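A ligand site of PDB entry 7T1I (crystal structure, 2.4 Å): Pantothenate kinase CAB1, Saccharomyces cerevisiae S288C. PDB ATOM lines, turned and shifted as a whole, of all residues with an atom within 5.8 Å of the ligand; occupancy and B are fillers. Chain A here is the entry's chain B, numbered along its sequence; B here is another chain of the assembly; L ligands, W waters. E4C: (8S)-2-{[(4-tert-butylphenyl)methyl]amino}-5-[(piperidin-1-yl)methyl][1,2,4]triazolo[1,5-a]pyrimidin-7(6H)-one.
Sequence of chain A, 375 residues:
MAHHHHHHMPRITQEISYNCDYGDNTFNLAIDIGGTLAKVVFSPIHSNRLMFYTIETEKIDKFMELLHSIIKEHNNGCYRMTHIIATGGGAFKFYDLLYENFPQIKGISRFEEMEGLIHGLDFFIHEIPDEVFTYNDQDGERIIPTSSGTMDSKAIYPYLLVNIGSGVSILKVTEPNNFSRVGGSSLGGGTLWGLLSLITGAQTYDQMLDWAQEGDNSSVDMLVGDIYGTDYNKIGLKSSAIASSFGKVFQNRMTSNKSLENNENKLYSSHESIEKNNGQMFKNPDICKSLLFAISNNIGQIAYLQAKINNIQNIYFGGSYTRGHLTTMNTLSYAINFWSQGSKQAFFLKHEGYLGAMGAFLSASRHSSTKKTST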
ATOM      1  N   VAL A 224     -12.193  22.306   9.667  1.00  0.00           N
ATOM      2  CA  VAL A 224     -11.224  21.714  10.571  1.00  0.00           C
ATOM      3  C   VAL A 224     -11.969  21.202  11.790  1.00  0.00           C
ATOM      4  O   VAL A 224     -11.767  20.067  12.211  1.00  0.00           O
ATOM      5  CB  VAL A 224     -10.097  22.691  10.965  1.00  0.00           C
ATOM      6  CG1 VAL A 224      -9.228  22.153  12.107  1.00  0.00           C
ATOM      7  CG2 VAL A 224      -9.220  23.069   9.770  1.00  0.00           C
ATOM      8  N   ILE A 227     -13.394  17.900  11.785  1.00  0.00           N
ATOM      9  CA  ILE A 227     -12.508  16.756  11.723  1.00  0.00           C
ATOM     10  C   ILE A 227     -11.867  16.523  13.104  1.00  0.00           C
ATOM     11  O   ILE A 227     -11.667  15.376  13.517  1.00  0.00           O
ATOM     12  CB  ILE A 227     -11.428  16.979  10.636  1.00  0.00           C
ATOM     13  CG1 ILE A 227     -12.060  17.171   9.250  1.00  0.00           C
ATOM     14  CG2 ILE A 227     -10.362  15.885  10.666  1.00  0.00           C
ATOM     15  CD1 ILE A 227     -11.069  17.553   8.144  1.00  0.00           C
ATOM     16  N   TYR A 228     -11.537  17.633  13.778  1.00  0.00           N
ATOM     17  CA  TYR A 228     -10.748  17.636  15.009  1.00  0.00           C
ATOM     18  C   TYR A 228     -11.602  17.910  16.251  1.00  0.00           C
ATOM     19  O   TYR A 228     -11.142  17.700  17.380  1.00  0.00           O
ATOM     20  CB  TYR A 228      -9.612  18.656  14.891  1.00  0.00           C
ATOM     21  CG  TYR A 228      -8.328  18.048  14.424  1.00  0.00           C
ATOM     22  CD1 TYR A 228      -8.053  17.872  13.066  1.00  0.00           C
ATOM     23  CD2 TYR A 228      -7.406  17.565  15.352  1.00  0.00           C
ATOM     24  CE1 TYR A 228      -6.874  17.272  12.653  1.00  0.00           C
ATOM     25  CE2 TYR A 228      -6.222  16.974  14.937  1.00  0.00           C
ATOM     26  CZ  TYR A 228      -5.961  16.808  13.593  1.00  0.00           C
ATOM     27  OH  TYR A 228      -4.792  16.197  13.215  1.00  0.00           O
ATOM     28  N   TYR A 232      -6.664  23.359  15.114  1.00  0.00           N
ATOM     29  CA  TYR A 232      -5.410  22.690  14.783  1.00  0.00           C
ATOM     30  C   TYR A 232      -4.316  23.749  14.638  1.00  0.00           C
ATOM     31  O   TYR A 232      -3.714  23.915  13.556  1.00  0.00           O
ATOM     32  CB  TYR A 232      -5.551  21.844  13.517  1.00  0.00           C
ATOM     33  CG  TYR A 232      -4.523  20.740  13.340  1.00  0.00           C
ATOM     34  CD1 TYR A 232      -3.409  20.663  14.158  1.00  0.00           C
ATOM     35  CD2 TYR A 232      -4.669  19.769  12.351  1.00  0.00           C
ATOM     36  CE1 TYR A 232      -2.462  19.661  13.996  1.00  0.00           C
ATOM     37  CE2 TYR A 232      -3.723  18.777  12.175  1.00  0.00           C
ATOM     38  CZ  TYR A 232      -2.608  18.712  13.000  1.00  0.00           C
ATOM     39  OH  TYR A 232      -1.663  17.735  12.840  1.00  0.00           O
ATOM     40  N   ILE A 235      -0.757  23.724  13.092  1.00  0.00           N
ATOM     41  CA  ILE A 235      -0.580  23.987  11.665  1.00  0.00           C
ATOM     42  C   ILE A 235      -1.171  25.349  11.296  1.00  0.00           C
ATOM     43  O   ILE A 235      -1.204  25.705  10.125  1.00  0.00           O
ATOM     44  CB  ILE A 235      -1.145  22.829  10.814  1.00  0.00           C
ATOM     45  CG1 ILE A 235      -2.687  22.789  10.804  1.00  0.00           C
ATOM     46  CG2 ILE A 235      -0.531  21.493  11.258  1.00  0.00           C
ATOM     47  CD1 ILE A 235      -3.324  21.843   9.797  1.00  0.00           C
ATOM     48  N   GLY A 236      -1.665  26.093  12.280  1.00  0.00           N
ATOM     49  CA  GLY A 236      -2.095  27.455  12.049  1.00  0.00           C
ATOM     50  C   GLY A 236      -3.495  27.507  11.440  1.00  0.00           C
ATOM     51  O   GLY A 236      -3.806  28.443  10.715  1.00  0.00           O
ATOM     52  N   LEU A 237      -4.321  26.513  11.756  1.00  0.00           N
ATOM     53  CA  LEU A 237      -5.676  26.499  11.218  1.00  0.00           C
ATOM     54  C   LEU A 237      -6.698  26.353  12.329  1.00  0.00           C
ATOM     55  O   LEU A 237      -6.574  25.498  13.200  1.00  0.00           O
ATOM     56  CB  LEU A 237      -5.836  25.387  10.177  1.00  0.00           C
ATOM     57  CG  LEU A 237      -5.043  25.571   8.881  1.00  0.00           C
ATOM     58  CD1 LEU A 237      -5.285  24.387   7.951  1.00  0.00           C
ATOM     59  CD2 LEU A 237      -5.414  26.865   8.184  1.00  0.00           C
ATOM     60  N   ALA A 241     -11.571  27.094   9.592  1.00  0.00           N
ATOM     61  CA  ALA A 241     -10.894  26.939   8.306  1.00  0.00           C
ATOM     62  C   ALA A 241     -11.506  25.802   7.499  1.00  0.00           C
ATOM     63  O   ALA A 241     -11.920  24.781   8.075  1.00  0.00           O
ATOM     64  CB  ALA A 241      -9.415  26.727   8.499  1.00  0.00           C
ATOM     65  N   ILE A 242     -11.541  26.000   6.163  1.00  0.00           N
ATOM     66  CA  ILE A 242     -12.125  25.072   5.211  1.00  0.00           C
ATOM     67  C   ILE A 242     -11.071  24.034   4.863  1.00  0.00           C
ATOM     68  O   ILE A 242     -10.033  24.345   4.274  1.00  0.00           O
ATOM     69  CB  ILE A 242     -12.701  25.790   3.962  1.00  0.00           C
ATOM     70  CG1 ILE A 242     -13.719  26.882   4.334  1.00  0.00           C
ATOM     71  CG2 ILE A 242     -13.295  24.811   2.958  1.00  0.00           C
ATOM     72  CD1 ILE A 242     -14.021  27.885   3.221  1.00  0.00           C
ATOM     73  N   ALA A 243     -11.370  22.786   5.236  1.00  0.00           N
ATOM     74  CA  ALA A 243     -10.456  21.684   5.001  1.00  0.00           C
ATOM     75  C   ALA A 243     -10.709  21.125   3.607  1.00  0.00           C
ATOM     76  O   ALA A 243      -9.777  20.829   2.862  1.00  0.00           O
ATOM     77  CB  ALA A 243     -10.651  20.649   6.082  1.00  0.00           C
ATOM     78  N   SER A 244     -11.983  21.008   3.231  1.00  0.00           N
ATOM     79  CA  SER A 244     -12.360  20.383   1.989  1.00  0.00           C
ATOM     80  C   SER A 244     -13.617  21.063   1.451  1.00  0.00           C
ATOM     81  O   SER A 244     -14.677  20.917   2.062  1.00  0.00           O
ATOM     82  CB  SER A 244     -12.646  18.934   2.251  1.00  0.00           C
ATOM     83  OG  SER A 244     -13.124  18.341   1.076  1.00  0.00           O
ATOM     84  N   PHE A 338      -3.602  36.312   4.931  1.00  0.00           N
ATOM     85  CA  PHE A 338      -3.493  35.122   5.753  1.00  0.00           C
ATOM     86  C   PHE A 338      -2.177  34.409   5.423  1.00  0.00           C
ATOM     87  O   PHE A 338      -1.420  34.066   6.327  1.00  0.00           O
ATOM     88  CB  PHE A 338      -4.713  34.219   5.548  1.00  0.00           C
ATOM     89  CG  PHE A 338      -4.797  33.027   6.476  1.00  0.00           C
ATOM     90  CD1 PHE A 338      -5.077  33.194   7.836  1.00  0.00           C
ATOM     91  CD2 PHE A 338      -4.587  31.735   6.025  1.00  0.00           C
ATOM     92  CE1 PHE A 338      -5.144  32.106   8.699  1.00  0.00           C
ATOM     93  CE2 PHE A 338      -4.662  30.642   6.899  1.00  0.00           C
ATOM     94  CZ  PHE A 338      -4.944  30.827   8.229  1.00  0.00           C
ATOM     95  N   TRP A 339      -1.944  34.176   4.128  1.00  0.00           N
ATOM     96  CA  TRP A 339      -0.842  33.295   3.771  1.00  0.00           C
ATOM     97  C   TRP A 339       0.479  34.000   4.058  1.00  0.00           C
ATOM     98  O   TRP A 339       1.460  33.319   4.323  1.00  0.00           O
ATOM     99  CB  TRP A 339      -0.928  32.807   2.315  1.00  0.00           C
ATOM    100  CG  TRP A 339      -1.784  31.608   2.098  1.00  0.00           C
ATOM    101  CD1 TRP A 339      -3.147  31.581   1.995  1.00  0.00           C
ATOM    102  CD2 TRP A 339      -1.337  30.236   1.927  1.00  0.00           C
ATOM    103  NE1 TRP A 339      -3.578  30.303   1.760  1.00  0.00           N
ATOM    104  CE2 TRP A 339      -2.502  29.453   1.717  1.00  0.00           C
ATOM    105  CE3 TRP A 339      -0.086  29.605   1.891  1.00  0.00           C
ATOM    106  CZ2 TRP A 339      -2.437  28.071   1.519  1.00  0.00           C
ATOM    107  CZ3 TRP A 339      -0.028  28.230   1.711  1.00  0.00           C
ATOM    108  CH2 TRP A 339      -1.190  27.480   1.501  1.00  0.00           C
ATOM    109  N   SER A 340       0.480  35.334   4.072  1.00  0.00           N
ATOM    110  CA  SER A 340       1.715  36.109   4.251  1.00  0.00           C
ATOM    111  C   SER A 340       1.760  36.723   5.660  1.00  0.00           C
ATOM    112  O   SER A 340       2.637  37.538   5.957  1.00  0.00           O
ATOM    113  CB  SER A 340       1.806  37.209   3.225  1.00  0.00           C
ATOM    114  OG  SER A 340       0.814  38.190   3.513  1.00  0.00           O
ATOM    115  N   GLN A 341       0.794  36.348   6.516  1.00  0.00           N
ATOM    116  CA  GLN A 341       0.721  36.941   7.852  1.00  0.00           C
ATOM    117  C   GLN A 341       0.799  38.470   7.730  1.00  0.00           C
ATOM    118  O   GLN A 341       1.558  39.103   8.467  1.00  0.00           O
ATOM    119  CB  GLN A 341       1.817  36.403   8.788  1.00  0.00           C
ATOM    120  CG  GLN A 341       1.641  34.945   9.186  1.00  0.00           C
ATOM    121  CD  GLN A 341       2.661  34.501  10.219  1.00  0.00           C
ATOM    122  OE1 GLN A 341       3.477  33.627   9.948  1.00  0.00           O
ATOM    123  NE2 GLN A 341       2.626  35.103  11.408  1.00  0.00           N
ATOM    124  N   GLU B 113      -0.701  14.178  13.935  1.00  0.00           N
ATOM    125  CA  GLU B 113      -1.081  13.755  12.607  1.00  0.00           C
ATOM    126  C   GLU B 113       0.053  13.966  11.596  1.00  0.00           C
ATOM    127  O   GLU B 113       0.322  13.068  10.799  1.00  0.00           O
ATOM    128  CB  GLU B 113      -2.395  14.397  12.131  1.00  0.00           C
ATOM    129  CG  GLU B 113      -2.882  13.792  10.814  1.00  0.00           C
ATOM    130  CD  GLU B 113      -4.090  14.401  10.107  1.00  0.00           C
ATOM    131  OE1 GLU B 113      -4.905  15.065  10.765  1.00  0.00           O
ATOM    132  OE2 GLU B 113      -4.205  14.204   8.879  1.00  0.00           O
ATOM    133  N   MET B 114       0.689  15.148  11.607  1.00  0.00           N
ATOM    134  CA  MET B 114       1.714  15.410  10.622  1.00  0.00           C
ATOM    135  C   MET B 114       2.950  14.540  10.902  1.00  0.00           C
ATOM    136  O   MET B 114       3.603  14.056   9.972  1.00  0.00           O
ATOM    137  CB  MET B 114       2.062  16.904  10.574  1.00  0.00           C
ATOM    138  CG  MET B 114       0.840  17.776  10.343  1.00  0.00           C
ATOM    139  SD  MET B 114       0.146  17.636   8.682  1.00  0.00           S
ATOM    140  CE  MET B 114      -1.582  17.270   9.021  1.00  0.00           C
ATOM    141  N   GLY B 167      -9.359  16.923   1.654  1.00  0.00           N
ATOM    142  CA  GLY B 167      -8.544  18.078   1.309  1.00  0.00           C
ATOM    143  C   GLY B 167      -7.114  17.623   1.076  1.00  0.00           C
ATOM    144  O   GLY B 167      -6.855  16.427   0.938  1.00  0.00           O
ATOM    145  N   VAL B 168      -6.197  18.600   1.083  1.00  0.00           N
ATOM    146  CA  VAL B 168      -4.817  18.351   0.716  1.00  0.00           C
ATOM    147  C   VAL B 168      -3.905  19.040   1.735  1.00  0.00           C
ATOM    148  O   VAL B 168      -4.135  20.193   2.075  1.00  0.00           O
ATOM    149  CB  VAL B 168      -4.538  18.833  -0.726  1.00  0.00           C
ATOM    150  CG1 VAL B 168      -3.081  18.647  -1.148  1.00  0.00           C
ATOM    151  CG2 VAL B 168      -5.483  18.186  -1.737  1.00  0.00           C
ATOM    152  N   SER B 169      -2.919  18.287   2.227  1.00  0.00           N
ATOM    153  CA  SER B 169      -1.871  18.843   3.059  1.00  0.00           C
ATOM    154  C   SER B 169      -0.544  18.608   2.338  1.00  0.00           C
ATOM    155  O   SER B 169      -0.365  17.581   1.691  1.00  0.00           O
ATOM    156  CB  SER B 169      -1.846  18.186   4.426  1.00  0.00           C
ATOM    157  OG  SER B 169      -2.960  18.553   5.221  1.00  0.00           O
ATOM    158  N   ARG B 181       4.435  21.200   7.952  1.00  0.00           N
ATOM    159  CA  ARG B 181       3.373  21.370   6.983  1.00  0.00           C
ATOM    160  C   ARG B 181       3.604  22.728   6.350  1.00  0.00           C
ATOM    161  O   ARG B 181       3.671  23.746   7.020  1.00  0.00           O
ATOM    162  CB  ARG B 181       1.999  21.230   7.661  1.00  0.00           C
ATOM    163  CG  ARG B 181       0.829  21.154   6.671  1.00  0.00           C
ATOM    164  CD  ARG B 181      -0.501  20.950   7.374  1.00  0.00           C
ATOM    165  NE  ARG B 181      -1.673  20.763   6.513  1.00  0.00           N
ATOM    166  CZ  ARG B 181      -2.383  21.755   5.931  1.00  0.00           C
ATOM    167  NH1 ARG B 181      -2.020  23.028   6.079  1.00  0.00           N
ATOM    168  NH2 ARG B 181      -3.436  21.456   5.169  1.00  0.00           N
ATOM    169  N   VAL B 182       3.817  22.760   5.063  1.00  0.00           N
ATOM    170  CA  VAL B 182       4.149  24.059   4.516  1.00  0.00           C
ATOM    171  C   VAL B 182       2.889  24.666   3.892  1.00  0.00           C
ATOM    172  O   VAL B 182       2.910  25.793   3.444  1.00  0.00           O
ATOM    173  CB  VAL B 182       5.297  23.939   3.497  1.00  0.00           C
ATOM    174  CG1 VAL B 182       6.623  23.645   4.193  1.00  0.00           C
ATOM    175  CG2 VAL B 182       4.970  22.897   2.423  1.00  0.00           C
ATOM    176  N   GLY B 183       1.790  23.930   3.863  1.00  0.00           N
ATOM    177  CA  GLY B 183       0.598  24.450   3.215  1.00  0.00           C
ATOM    178  C   GLY B 183      -0.388  23.323   2.964  1.00  0.00           C
ATOM    179  O   GLY B 183      -0.162  22.192   3.413  1.00  0.00           O
ATOM    180  N   GLY B 184      -1.487  23.633   2.255  1.00  0.00           N
ATOM    181  CA  GLY B 184      -2.552  22.696   1.944  1.00  0.00           C
ATOM    182  C   GLY B 184      -3.613  23.368   1.081  1.00  0.00           C
ATOM    183  O   GLY B 184      -3.511  24.547   0.761  1.00  0.00           O
ATOM    184  N   SER B 185      -4.665  22.642   0.708  1.00  0.00           N
ATOM    185  CA  SER B 185      -5.628  23.261  -0.160  1.00  0.00           C
ATOM    186  C   SER B 185      -6.941  22.543   0.082  1.00  0.00           C
ATOM    187  O   SER B 185      -6.942  21.326   0.303  1.00  0.00           O
ATOM    188  CB  SER B 185      -5.216  23.102  -1.592  1.00  0.00           C
ATOM    189  OG  SER B 185      -6.342  23.189  -2.451  1.00  0.00           O
ATOM    190  N   SER B 186      -8.026  23.324  -0.019  1.00  0.00           N
ATOM    191  CA  SER B 186      -9.362  22.837   0.231  1.00  0.00           C
ATOM    192  C   SER B 186      -9.916  22.156  -1.012  1.00  0.00           C
ATOM    193  O   SER B 186     -11.027  21.615  -0.961  1.00  0.00           O
ATOM    194  CB  SER B 186     -10.253  23.945   0.726  1.00  0.00           C
ATOM    195  OG  SER B 186     -10.728  24.746  -0.356  1.00  0.00           O
HETATM  196  C20 E4C L   1      -7.012  21.527   5.984  1.00  0.00           C
HETATM  197  C28 E4C L   1      -6.311  19.634   4.740  1.00  0.00           C
HETATM  198  C21 E4C L   1      -6.971  20.798   7.149  1.00  0.00           C
HETATM  199  C27 E4C L   1      -6.277  18.885   5.899  1.00  0.00           C
HETATM  200  C19 E4C L   1      -6.692  20.955   4.773  1.00  0.00           C
HETATM  201  C22 E4C L   1      -6.621  19.459   7.113  1.00  0.00           C
HETATM  202  C16 E4C L   1      -6.326  24.052   3.836  1.00  0.00           C
HETATM  203  C4  E4C L   1      -4.470  24.978   4.398  1.00  0.00           C
HETATM  204  C14 E4C L   1      -3.976  27.735   4.622  1.00  0.00           C
HETATM  205  C6  E4C L   1      -3.030  26.803   4.857  1.00  0.00           C
HETATM  206  C2  E4C L   1      -5.330  27.250   4.256  1.00  0.00           C
HETATM  207  C11 E4C L   1       0.032  29.983   8.320  1.00  0.00           C
HETATM  208  C10 E4C L   1      -1.226  29.164   8.604  1.00  0.00           C
HETATM  209  C12 E4C L   1      -0.208  30.381   6.870  1.00  0.00           C
HETATM  210  C9  E4C L   1      -1.494  27.994   7.616  1.00  0.00           C
HETATM  211  C13 E4C L   1      -0.260  29.219   5.857  1.00  0.00           C
HETATM  212  C24 E4C L   1      -7.270  19.382   9.545  1.00  0.00           C
HETATM  213  C25 E4C L   1      -5.166  18.331   8.741  1.00  0.00           C
HETATM  214  C26 E4C L   1      -7.352  17.348   8.120  1.00  0.00           C
HETATM  215  C18 E4C L   1      -6.715  21.700   3.508  1.00  0.00           C
HETATM  216  C7  E4C L   1      -1.644  27.271   5.217  1.00  0.00           C
HETATM  217  C23 E4C L   1      -6.591  18.631   8.388  1.00  0.00           C
HETATM  218  N15 E4C L   1      -5.012  23.784   4.176  1.00  0.00           N
HETATM  219  N29 E4C L   1      -6.645  25.352   3.818  1.00  0.00           N
HETATM  220  N3  E4C L   1      -5.460  25.902   4.175  1.00  0.00           N
HETATM  221  N5  E4C L   1      -3.229  25.420   4.766  1.00  0.00           N
HETATM  222  N17 E4C L   1      -7.192  23.055   3.575  1.00  0.00           N
HETATM  223  N8  E4C L   1      -1.467  28.399   6.158  1.00  0.00           N
HETATM  224  O1  E4C L   1      -6.340  27.924   3.997  1.00  0.00           O
HETATM  225  O   HOH W   1      -9.170  26.759   3.697  1.00  0.00           O
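The guanidinium group of Arg 181 of chain B is in hydrogen-bond range of the backbone carbonyl oxygen of Val 168 of chain B, 3.4 Å away. The side-chain hydroxyl (OG) of Ser 169 of chain B is in hydrogen-bond range of the guanidinium group (NE) of Arg 181 of chain B (2.9 Å). The guanidinium group (NH1) of Arg 181 of chain B lies within hydrogen-bond range of the backbone carbonyl oxygen (O) of Gly 183 of chain B, at 3.4 Å. N of Ser 185 of chain B sits at hydrogen-bond distance from O of Val 168 of chain B (2.9 Å). N of Tyr 232 sits at hydrogen-bond distance from O of Leu 237, 2.9 Å away. The side-chain hydroxyl (OH) of Tyr 228 sits at hydrogen-bond distance from the side-chain carboxylate (OE1) of Glu 113 of chain B (2.7 Å).
Merely in contact with the ligand: Ser 185 of chain B (3.2 Å), Val 168 of chain B (3.3 Å), Ser 169 of chain B (3.4 Å), Ile 235 (3.4 Å), Gly 236 (3.4 Å), Gly 184 of chain B (3.4 Å), Trp 339 (3.5 Å), Leu 237 (3.7 Å), Ser 186 of chain B (3.7 Å), Ile 227 (3.7 Å), Met 114 of chain B (3.7 Å), Tyr 232 (3.8 Å), Phe 338 (3.8 Å), Tyr 228 (3.8 Å), Glu 113 of chain B (3.9 Å) and Gly 183 of chain B (3.96 Å). Hydrophobic or aromatic side chains that line the ligand: Ile 227, Tyr 228, Tyr 232, Leu 237, Ala 243, Phe 338, Trp 339 and Met 114 of chain B. 19 residues have an atom within 4 Å of the ligand: Ile 227, Tyr 228, Tyr 232, Ile 235, Gly 236, Leu 237, Ile 242, Ala 243, Phe 338, Trp 339, Glu 113 of chain B, Met 114 of chain B, Val 168 of chain B, Ser 169 of chain B, Arg 181 of chain B, Gly 183 of chain B, Gly 184 of chain B, Ser 185 of chain B and Ser 186 of chain B. Along chain A the residues within 4 Å of the ligand span positions 227 to 339. The nearest printed residue that does not touch the ligand is Val 224 (4.1 Å).
Water W1 lies within hydrogen-bond range of the backbone carbonyl oxygen (O) of Ile 242 (2.6 Å) and a nitrogen (N29) of the ligand (2.9 Å).
The guanidinium group (NH2) of Arg 181 of chain B is in hydrogen-bond range of a nitrogen (N15) of the ligand. N17 of the ligand lies within hydrogen-bond range of O of Ile 242, 3.2 Å away. The backbone carbonyl oxygen of Ala 243 lies close to a nitrogen (N17) of the ligand (3.5 Å).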
